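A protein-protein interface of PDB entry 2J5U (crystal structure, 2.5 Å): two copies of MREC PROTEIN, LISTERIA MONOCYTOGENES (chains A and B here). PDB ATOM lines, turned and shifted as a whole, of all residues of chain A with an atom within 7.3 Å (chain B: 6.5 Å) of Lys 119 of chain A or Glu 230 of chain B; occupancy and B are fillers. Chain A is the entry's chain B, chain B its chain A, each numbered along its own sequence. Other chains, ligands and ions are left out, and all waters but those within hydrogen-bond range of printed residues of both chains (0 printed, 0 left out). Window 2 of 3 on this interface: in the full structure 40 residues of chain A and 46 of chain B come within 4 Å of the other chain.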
ATOM      1  N   VAL A  75      -4.867 -18.369 -16.930  1.00  0.00           N
ATOM      2  CA  VAL A  75      -5.267 -18.844 -15.618  1.00  0.00           C
ATOM      3  C   VAL A  75      -4.387 -20.074 -15.462  1.00  0.00           C
ATOM      4  O   VAL A  75      -4.360 -20.932 -16.344  1.00  0.00           O
ATOM      5  CB  VAL A  75      -6.728 -19.285 -15.577  1.00  0.00           C
ATOM      6  CG1 VAL A  75      -7.032 -19.881 -14.221  1.00  0.00           C
ATOM      7  CG2 VAL A  75      -7.635 -18.114 -15.839  1.00  0.00           C
ATOM      8  N   ILE A  76      -3.648 -20.161 -14.368  1.00  0.00           N
ATOM      9  CA  ILE A  76      -2.767 -21.299 -14.182  1.00  0.00           C
ATOM     10  C   ILE A  76      -3.204 -22.175 -13.035  1.00  0.00           C
ATOM     11  O   ILE A  76      -2.622 -23.228 -12.800  1.00  0.00           O
ATOM     12  CB  ILE A  76      -1.331 -20.853 -13.888  1.00  0.00           C
ATOM     13  CG1 ILE A  76      -1.314 -20.003 -12.617  1.00  0.00           C
ATOM     14  CG2 ILE A  76      -0.774 -20.098 -15.073  1.00  0.00           C
ATOM     15  CD1 ILE A  76       0.064 -19.657 -12.121  1.00  0.00           C
ATOM     16  N   SER A  77      -4.229 -21.755 -12.314  1.00  0.00           N
ATOM     17  CA  SER A  77      -4.659 -22.548 -11.185  1.00  0.00           C
ATOM     18  C   SER A  77      -6.031 -22.169 -10.665  1.00  0.00           C
ATOM     19  O   SER A  77      -6.366 -20.998 -10.565  1.00  0.00           O
ATOM     20  CB  SER A  77      -3.631 -22.403 -10.076  1.00  0.00           C
ATOM     21  OG  SER A  77      -4.105 -22.990  -8.888  1.00  0.00           O
ATOM     22  N   GLU A  88      -6.014 -18.054 -10.300  1.00  0.00           N
ATOM     23  CA  GLU A  88      -4.636 -17.588 -10.272  1.00  0.00           C
ATOM     24  C   GLU A  88      -4.093 -17.377 -11.686  1.00  0.00           C
ATOM     25  O   GLU A  88      -4.264 -18.233 -12.557  1.00  0.00           O
ATOM     26  CB  GLU A  88      -3.777 -18.597  -9.529  1.00  0.00           C
ATOM     27  CG  GLU A  88      -2.426 -18.063  -9.134  1.00  0.00           C
ATOM     28  CD  GLU A  88      -1.687 -19.020  -8.218  1.00  0.00           C
ATOM     29  OE1 GLU A  88      -0.601 -18.652  -7.708  1.00  0.00           O
ATOM     30  OE2 GLU A  88      -2.201 -20.146  -8.014  1.00  0.00           O
ATOM     31  N   ILE A  89      -3.437 -16.242 -11.915  1.00  0.00           N
ATOM     32  CA  ILE A  89      -2.890 -15.935 -13.230  1.00  0.00           C
ATOM     33  C   ILE A  89      -1.371 -15.915 -13.224  1.00  0.00           C
ATOM     34  O   ILE A  89      -0.753 -15.685 -12.186  1.00  0.00           O
ATOM     35  CB  ILE A  89      -3.419 -14.585 -13.746  1.00  0.00           C
ATOM     36  CG1 ILE A  89      -3.050 -13.467 -12.769  1.00  0.00           C
ATOM     37  CG2 ILE A  89      -4.933 -14.665 -13.926  1.00  0.00           C
ATOM     38  CD1 ILE A  89      -3.410 -12.080 -13.262  1.00  0.00           C
ATOM     39  N   ASP A  90      -0.781 -16.152 -14.395  1.00  0.00           N
ATOM     40  CA  ASP A  90       0.673 -16.210 -14.553  1.00  0.00           C
ATOM     41  C   ASP A  90       1.392 -14.871 -14.733  1.00  0.00           C
ATOM     42  O   ASP A  90       2.429 -14.801 -15.401  1.00  0.00           O
ATOM     43  CB  ASP A  90       1.029 -17.116 -15.734  1.00  0.00           C
ATOM     44  CG  ASP A  90       0.524 -16.567 -17.050  1.00  0.00           C
ATOM     45  OD1 ASP A  90       0.861 -17.129 -18.120  1.00  0.00           O
ATOM     46  OD2 ASP A  90      -0.223 -15.566 -17.007  1.00  0.00           O
ATOM     47  N   LYS A  91       0.842 -13.812 -14.156  1.00  0.00           N
ATOM     48  CA  LYS A  91       1.470 -12.498 -14.229  1.00  0.00           C
ATOM     49  C   LYS A  91       1.394 -11.913 -12.831  1.00  0.00           C
ATOM     50  O   LYS A  91       0.400 -12.099 -12.122  1.00  0.00           O
ATOM     51  CB  LYS A  91       0.759 -11.601 -15.250  1.00  0.00           C
ATOM     52  CG  LYS A  91       0.972 -12.047 -16.702  1.00  0.00           C
ATOM     53  CD  LYS A  91       2.429 -11.892 -17.109  1.00  0.00           C
ATOM     54  CE  LYS A  91       2.853 -12.912 -18.167  1.00  0.00           C
ATOM     55  NZ  LYS A  91       2.114 -12.783 -19.450  1.00  0.00           N
ATOM     56  N   GLY A  92       2.458 -11.234 -12.418  1.00  0.00           N
ATOM     57  CA  GLY A  92       2.473 -10.660 -11.088  1.00  0.00           C
ATOM     58  C   GLY A  92       3.291  -9.393 -10.934  1.00  0.00           C
ATOM     59  O   GLY A  92       3.445  -8.595 -11.864  1.00  0.00           O
ATOM     60  N   SER A  93       3.806  -9.220  -9.724  1.00  0.00           N
ATOM     61  CA  SER A  93       4.619  -8.071  -9.347  1.00  0.00           C
ATOM     62  C   SER A  93       5.551  -7.591 -10.458  1.00  0.00           C
ATOM     63  O   SER A  93       5.386  -6.493 -10.986  1.00  0.00           O
ATOM     64  CB  SER A  93       5.436  -8.426  -8.101  1.00  0.00           C
ATOM     65  OG  SER A  93       6.225  -7.337  -7.683  1.00  0.00           O
ATOM     66  N   SER A  94       6.522  -8.424 -10.809  1.00  0.00           N
ATOM     67  CA  SER A  94       7.498  -8.095 -11.842  1.00  0.00           C
ATOM     68  C   SER A  94       6.926  -7.841 -13.238  1.00  0.00           C
ATOM     69  O   SER A  94       7.687  -7.713 -14.198  1.00  0.00           O
ATOM     70  CB  SER A  94       8.528  -9.214 -11.941  1.00  0.00           C
ATOM     71  OG  SER A  94       7.914 -10.401 -12.418  1.00  0.00           O
ATOM     72  N   ASP A  95       5.604  -7.778 -13.367  1.00  0.00           N
ATOM     73  CA  ASP A  95       4.985  -7.537 -14.674  1.00  0.00           C
ATOM     74  C   ASP A  95       4.123  -6.285 -14.638  1.00  0.00           C
ATOM     75  O   ASP A  95       3.505  -5.900 -15.637  1.00  0.00           O
ATOM     76  CB  ASP A  95       4.130  -8.734 -15.102  1.00  0.00           C
ATOM     77  CG  ASP A  95       4.943 -10.008 -15.261  1.00  0.00           C
ATOM     78  OD1 ASP A  95       4.898 -10.864 -14.344  1.00  0.00           O
ATOM     79  OD2 ASP A  95       5.631 -10.144 -16.301  1.00  0.00           O
ATOM     80  N   THR A 116      -0.629 -10.346  -4.737  1.00  0.00           N
ATOM     81  CA  THR A 116       0.298 -10.457  -5.857  1.00  0.00           C
ATOM     82  C   THR A 116       1.627 -11.057  -5.442  1.00  0.00           C
ATOM     83  O   THR A 116       2.116 -10.809  -4.340  1.00  0.00           O
ATOM     84  CB  THR A 116       0.614  -9.090  -6.461  1.00  0.00           C
ATOM     85  OG1 THR A 116      -0.605  -8.426  -6.790  1.00  0.00           O
ATOM     86  CG2 THR A 116       1.441  -9.246  -7.718  1.00  0.00           C
ATOM     87  N   GLY A 117       2.211 -11.834  -6.348  1.00  0.00           N
ATOM     88  CA  GLY A 117       3.492 -12.459  -6.095  1.00  0.00           C
ATOM     89  C   GLY A 117       4.462 -11.975  -7.149  1.00  0.00           C
ATOM     90  O   GLY A 117       4.165 -11.042  -7.885  1.00  0.00           O
ATOM     91  N   ALA A 118       5.614 -12.615  -7.247  1.00  0.00           N
ATOM     92  CA  ALA A 118       6.609 -12.197  -8.215  1.00  0.00           C
ATOM     93  C   ALA A 118       6.195 -12.440  -9.653  1.00  0.00           C
ATOM     94  O   ALA A 118       6.156 -11.510 -10.458  1.00  0.00           O
ATOM     95  CB  ALA A 118       7.925 -12.903  -7.934  1.00  0.00           C
ATOM     96  N   LYS A 119       5.886 -13.699  -9.963  1.00  0.00           N
ATOM     97  CA  LYS A 119       5.516 -14.114 -11.318  1.00  0.00           C
ATOM     98  C   LYS A 119       4.044 -14.522 -11.499  1.00  0.00           C
ATOM     99  O   LYS A 119       3.650 -14.998 -12.567  1.00  0.00           O
ATOM    100  CB  LYS A 119       6.426 -15.273 -11.736  1.00  0.00           C
ATOM    101  CG  LYS A 119       7.903 -14.901 -11.863  1.00  0.00           C
ATOM    102  CD  LYS A 119       8.176 -14.302 -13.227  1.00  0.00           C
ATOM    103  CE  LYS A 119       7.834 -15.313 -14.312  1.00  0.00           C
ATOM    104  NZ  LYS A 119       7.963 -14.757 -15.680  1.00  0.00           N
ATOM    105  N   SER A 120       3.235 -14.333 -10.461  1.00  0.00           N
ATOM    106  CA  SER A 120       1.825 -14.695 -10.535  1.00  0.00           C
ATOM    107  C   SER A 120       0.966 -13.836  -9.614  1.00  0.00           C
ATOM    108  O   SER A 120       1.475 -12.961  -8.914  1.00  0.00           O
ATOM    109  CB  SER A 120       1.645 -16.160 -10.150  1.00  0.00           C
ATOM    110  OG  SER A 120       1.814 -16.332  -8.756  1.00  0.00           O
ATOM    111  N   ALA A 121      -0.336 -14.101  -9.611  1.00  0.00           N
ATOM    112  CA  ALA A 121      -1.257 -13.353  -8.771  1.00  0.00           C
ATOM    113  C   ALA A 121      -2.624 -14.014  -8.684  1.00  0.00           C
ATOM    114  O   ALA A 121      -3.003 -14.808  -9.544  1.00  0.00           O
ATOM    115  CB  ALA A 121      -1.406 -11.933  -9.294  1.00  0.00           C
ATOM    116  N   ASP B  63       4.285 -19.197 -22.604  1.00  0.00           N
ATOM    117  CA  ASP B  63       4.072 -20.322 -21.702  1.00  0.00           C
ATOM    118  C   ASP B  63       2.618 -20.475 -21.306  1.00  0.00           C
ATOM    119  O   ASP B  63       2.276 -20.388 -20.124  1.00  0.00           O
ATOM    120  CB  ASP B  63       4.926 -20.149 -20.443  1.00  0.00           C
ATOM    121  CG  ASP B  63       6.413 -20.092 -20.754  1.00  0.00           C
ATOM    122  OD1 ASP B  63       6.914 -21.024 -21.426  1.00  0.00           O
ATOM    123  OD2 ASP B  63       7.079 -19.121 -20.330  1.00  0.00           O
ATOM    124  N   SER B  64       1.765 -20.697 -22.302  1.00  0.00           N
ATOM    125  CA  SER B  64       0.347 -20.876 -22.050  1.00  0.00           C
ATOM    126  C   SER B  64       0.142 -22.178 -21.273  1.00  0.00           C
ATOM    127  O   SER B  64       1.065 -22.975 -21.101  1.00  0.00           O
ATOM    128  CB  SER B  64      -0.433 -20.939 -23.359  1.00  0.00           C
ATOM    129  OG  SER B  64      -0.322 -22.222 -23.937  1.00  0.00           O
ATOM    130  N   GLY B 183      -2.443 -27.101 -11.183  1.00  0.00           N
ATOM    131  CA  GLY B 183      -1.146 -26.455 -11.150  1.00  0.00           C
ATOM    132  C   GLY B 183       0.085 -27.262 -11.498  1.00  0.00           C
ATOM    133  O   GLY B 183       1.191 -26.726 -11.458  1.00  0.00           O
ATOM    134  N   ARG B 227       5.800 -29.242 -17.311  1.00  0.00           N
ATOM    135  CA  ARG B 227       4.781 -28.226 -17.591  1.00  0.00           C
ATOM    136  C   ARG B 227       5.451 -26.874 -17.787  1.00  0.00           C
ATOM    137  O   ARG B 227       6.318 -26.496 -16.999  1.00  0.00           O
ATOM    138  CB  ARG B 227       3.769 -28.157 -16.440  1.00  0.00           C
ATOM    139  CG  ARG B 227       2.956 -26.883 -16.378  1.00  0.00           C
ATOM    140  CD  ARG B 227       1.905 -26.996 -15.306  1.00  0.00           C
ATOM    141  NE  ARG B 227       1.421 -25.698 -14.856  1.00  0.00           N
ATOM    142  CZ  ARG B 227       0.165 -25.462 -14.497  1.00  0.00           C
ATOM    143  NH1 ARG B 227      -0.200 -24.254 -14.090  1.00  0.00           N
ATOM    144  NH2 ARG B 227      -0.733 -26.435 -14.563  1.00  0.00           N
ATOM    145  N   SER B 228       5.059 -26.152 -18.834  1.00  0.00           N
ATOM    146  CA  SER B 228       5.658 -24.843 -19.108  1.00  0.00           C
ATOM    147  C   SER B 228       5.023 -23.750 -18.275  1.00  0.00           C
ATOM    148  O   SER B 228       5.712 -22.913 -17.712  1.00  0.00           O
ATOM    149  CB  SER B 228       5.518 -24.469 -20.584  1.00  0.00           C
ATOM    150  OG  SER B 228       6.218 -25.376 -21.406  1.00  0.00           O
ATOM    151  N   ALA B 229       3.701 -23.759 -18.209  1.00  0.00           N
ATOM    152  CA  ALA B 229       2.996 -22.754 -17.451  1.00  0.00           C
ATOM    153  C   ALA B 229       3.495 -22.682 -16.019  1.00  0.00           C
ATOM    154  O   ALA B 229       3.886 -23.692 -15.432  1.00  0.00           O
ATOM    155  CB  ALA B 229       1.510 -23.048 -17.466  1.00  0.00           C
ATOM    156  N   GLU B 230       3.485 -21.469 -15.476  1.00  0.00           N
ATOM    157  CA  GLU B 230       3.895 -21.222 -14.104  1.00  0.00           C
ATOM    158  C   GLU B 230       3.125 -22.176 -13.194  1.00  0.00           C
ATOM    159  O   GLU B 230       1.979 -22.525 -13.479  1.00  0.00           O
ATOM    160  CB  GLU B 230       3.559 -19.779 -13.740  1.00  0.00           C
ATOM    161  CG  GLU B 230       3.839 -19.393 -12.303  1.00  0.00           C
ATOM    162  CD  GLU B 230       5.313 -19.233 -12.018  1.00  0.00           C
ATOM    163  OE1 GLU B 230       5.646 -18.757 -10.914  1.00  0.00           O
ATOM    164  OE2 GLU B 230       6.141 -19.582 -12.891  1.00  0.00           O
ATOM    165  N   ALA B 231       3.744 -22.592 -12.098  1.00  0.00           N
ATOM    166  CA  ALA B 231       3.093 -23.511 -11.173  1.00  0.00           C
ATOM    167  C   ALA B 231       2.028 -22.810 -10.348  1.00  0.00           C
ATOM    168  O   ALA B 231       2.181 -21.644  -9.975  1.00  0.00           O
ATOM    169  CB  ALA B 231       4.120 -24.138 -10.257  1.00  0.00           C
ATOM    170  N   GLY B 232       0.951 -23.534 -10.056  1.00  0.00           N
ATOM    171  CA  GLY B 232      -0.127 -22.964  -9.274  1.00  0.00           C
ATOM    172  C   GLY B 232      -0.132 -23.414  -7.825  1.00  0.00           C
ATOM    173  O   GLY B 232       0.070 -24.595  -7.526  1.00  0.00           O
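No position is printed for both chains.
Of the 9 printed residues of chain B, 5 touch a printed residue of chain A.
Of the 17 printed residues of chain A, 4 touch a printed residue of chain B.
Printed residues of chain A that touch a printed residue of chain B: Ile 76, Ser 77, Glu 88 and Lys 119.
Hydrophobic or aromatic side chains of chain A that line the printed part of chain B: Ile 76.
Along chain A the printed residues that touch a printed residue of chain B span positions 76 to 119.
Among the printed residues, no Asp or Glu carboxylate lies within 4 Å of a Lys or Arg side-chain nitrogen of the other chain.
Among the printed residues, merely in contact across the chains: Ile 76 of chain A with Gly 183 of chain B (3.9 Å), Ile 76 of chain A with Glu 230 of chain B (3.7 Å), Ile 76 of chain A with Ala 231 of chain B (3.6 Å), Ser 77 of chain A with Gly 232 of chain B (3.6 Å), Glu 88 of chain A with Gly 232 of chain B (3.7 Å) and Lys 119 of chain A with Glu 230 of chain B (3.7 Å).
O of Gly 183 of chain B lies within hydrogen-bond range of N of Gly 232 of chain B (3.5 Å).
The guanidinium group (NE) of Arg 227 of chain B is in hydrogen-bond range of the backbone carbonyl oxygen (O) of Ala 229 of chain B, 3.2 Å away.
The guanidinium group (NH1) of Arg 227 of chain B is in hydrogen-bond range of the backbone carbonyl oxygen (O) of Glu 230 of chain B (2.8 Å).
N of Ile 76 of chain A sits at hydrogen-bond distance from O of Glu 88 of chain A (2.7 Å).
The backbone NH (N) of Glu 88 of chain A is in hydrogen-bond range of the backbone carbonyl oxygen (O) of Ser 77 of chain A, 3.0 Å away.
The backbone carbonyl oxygen (O) of Lys 119 of chain A sits at hydrogen-bond distance from the backbone NH (N) of Lys 91 of chain A.
Lys 119 of chain A touches one residue of chain B.
Printed residues of chain A within 4 Å of Gly 232 of chain B: Ser 77 (3.6 Å) and Glu 88 (3.7 Å).
Of the printed residues of chain B, Ser 77 of chain A touches Gly 232.
Of the printed residues of chain A, Arg 227 of chain B touches Ile 76.
Printed residues of chain B within 4 Å of Glu 88 of chain A: Gly 232 (3.7 Å).
Printed residues of chain A within 4 Å of Gly 183 of chain B: Ile 76.
Ser 93 of chain A touches none of the printed residues of chain B.
Asp 95 of chain A touches none of the printed residues of chain B.
The nearest residue of chain A that does not touch Glu 230 of chain B is Asp 90 of chain A (4.2 Å).
NH1 of Arg 227 of chain B is in hydrogen-bond range of O of Ile 76 of chain A (2.9 Å).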
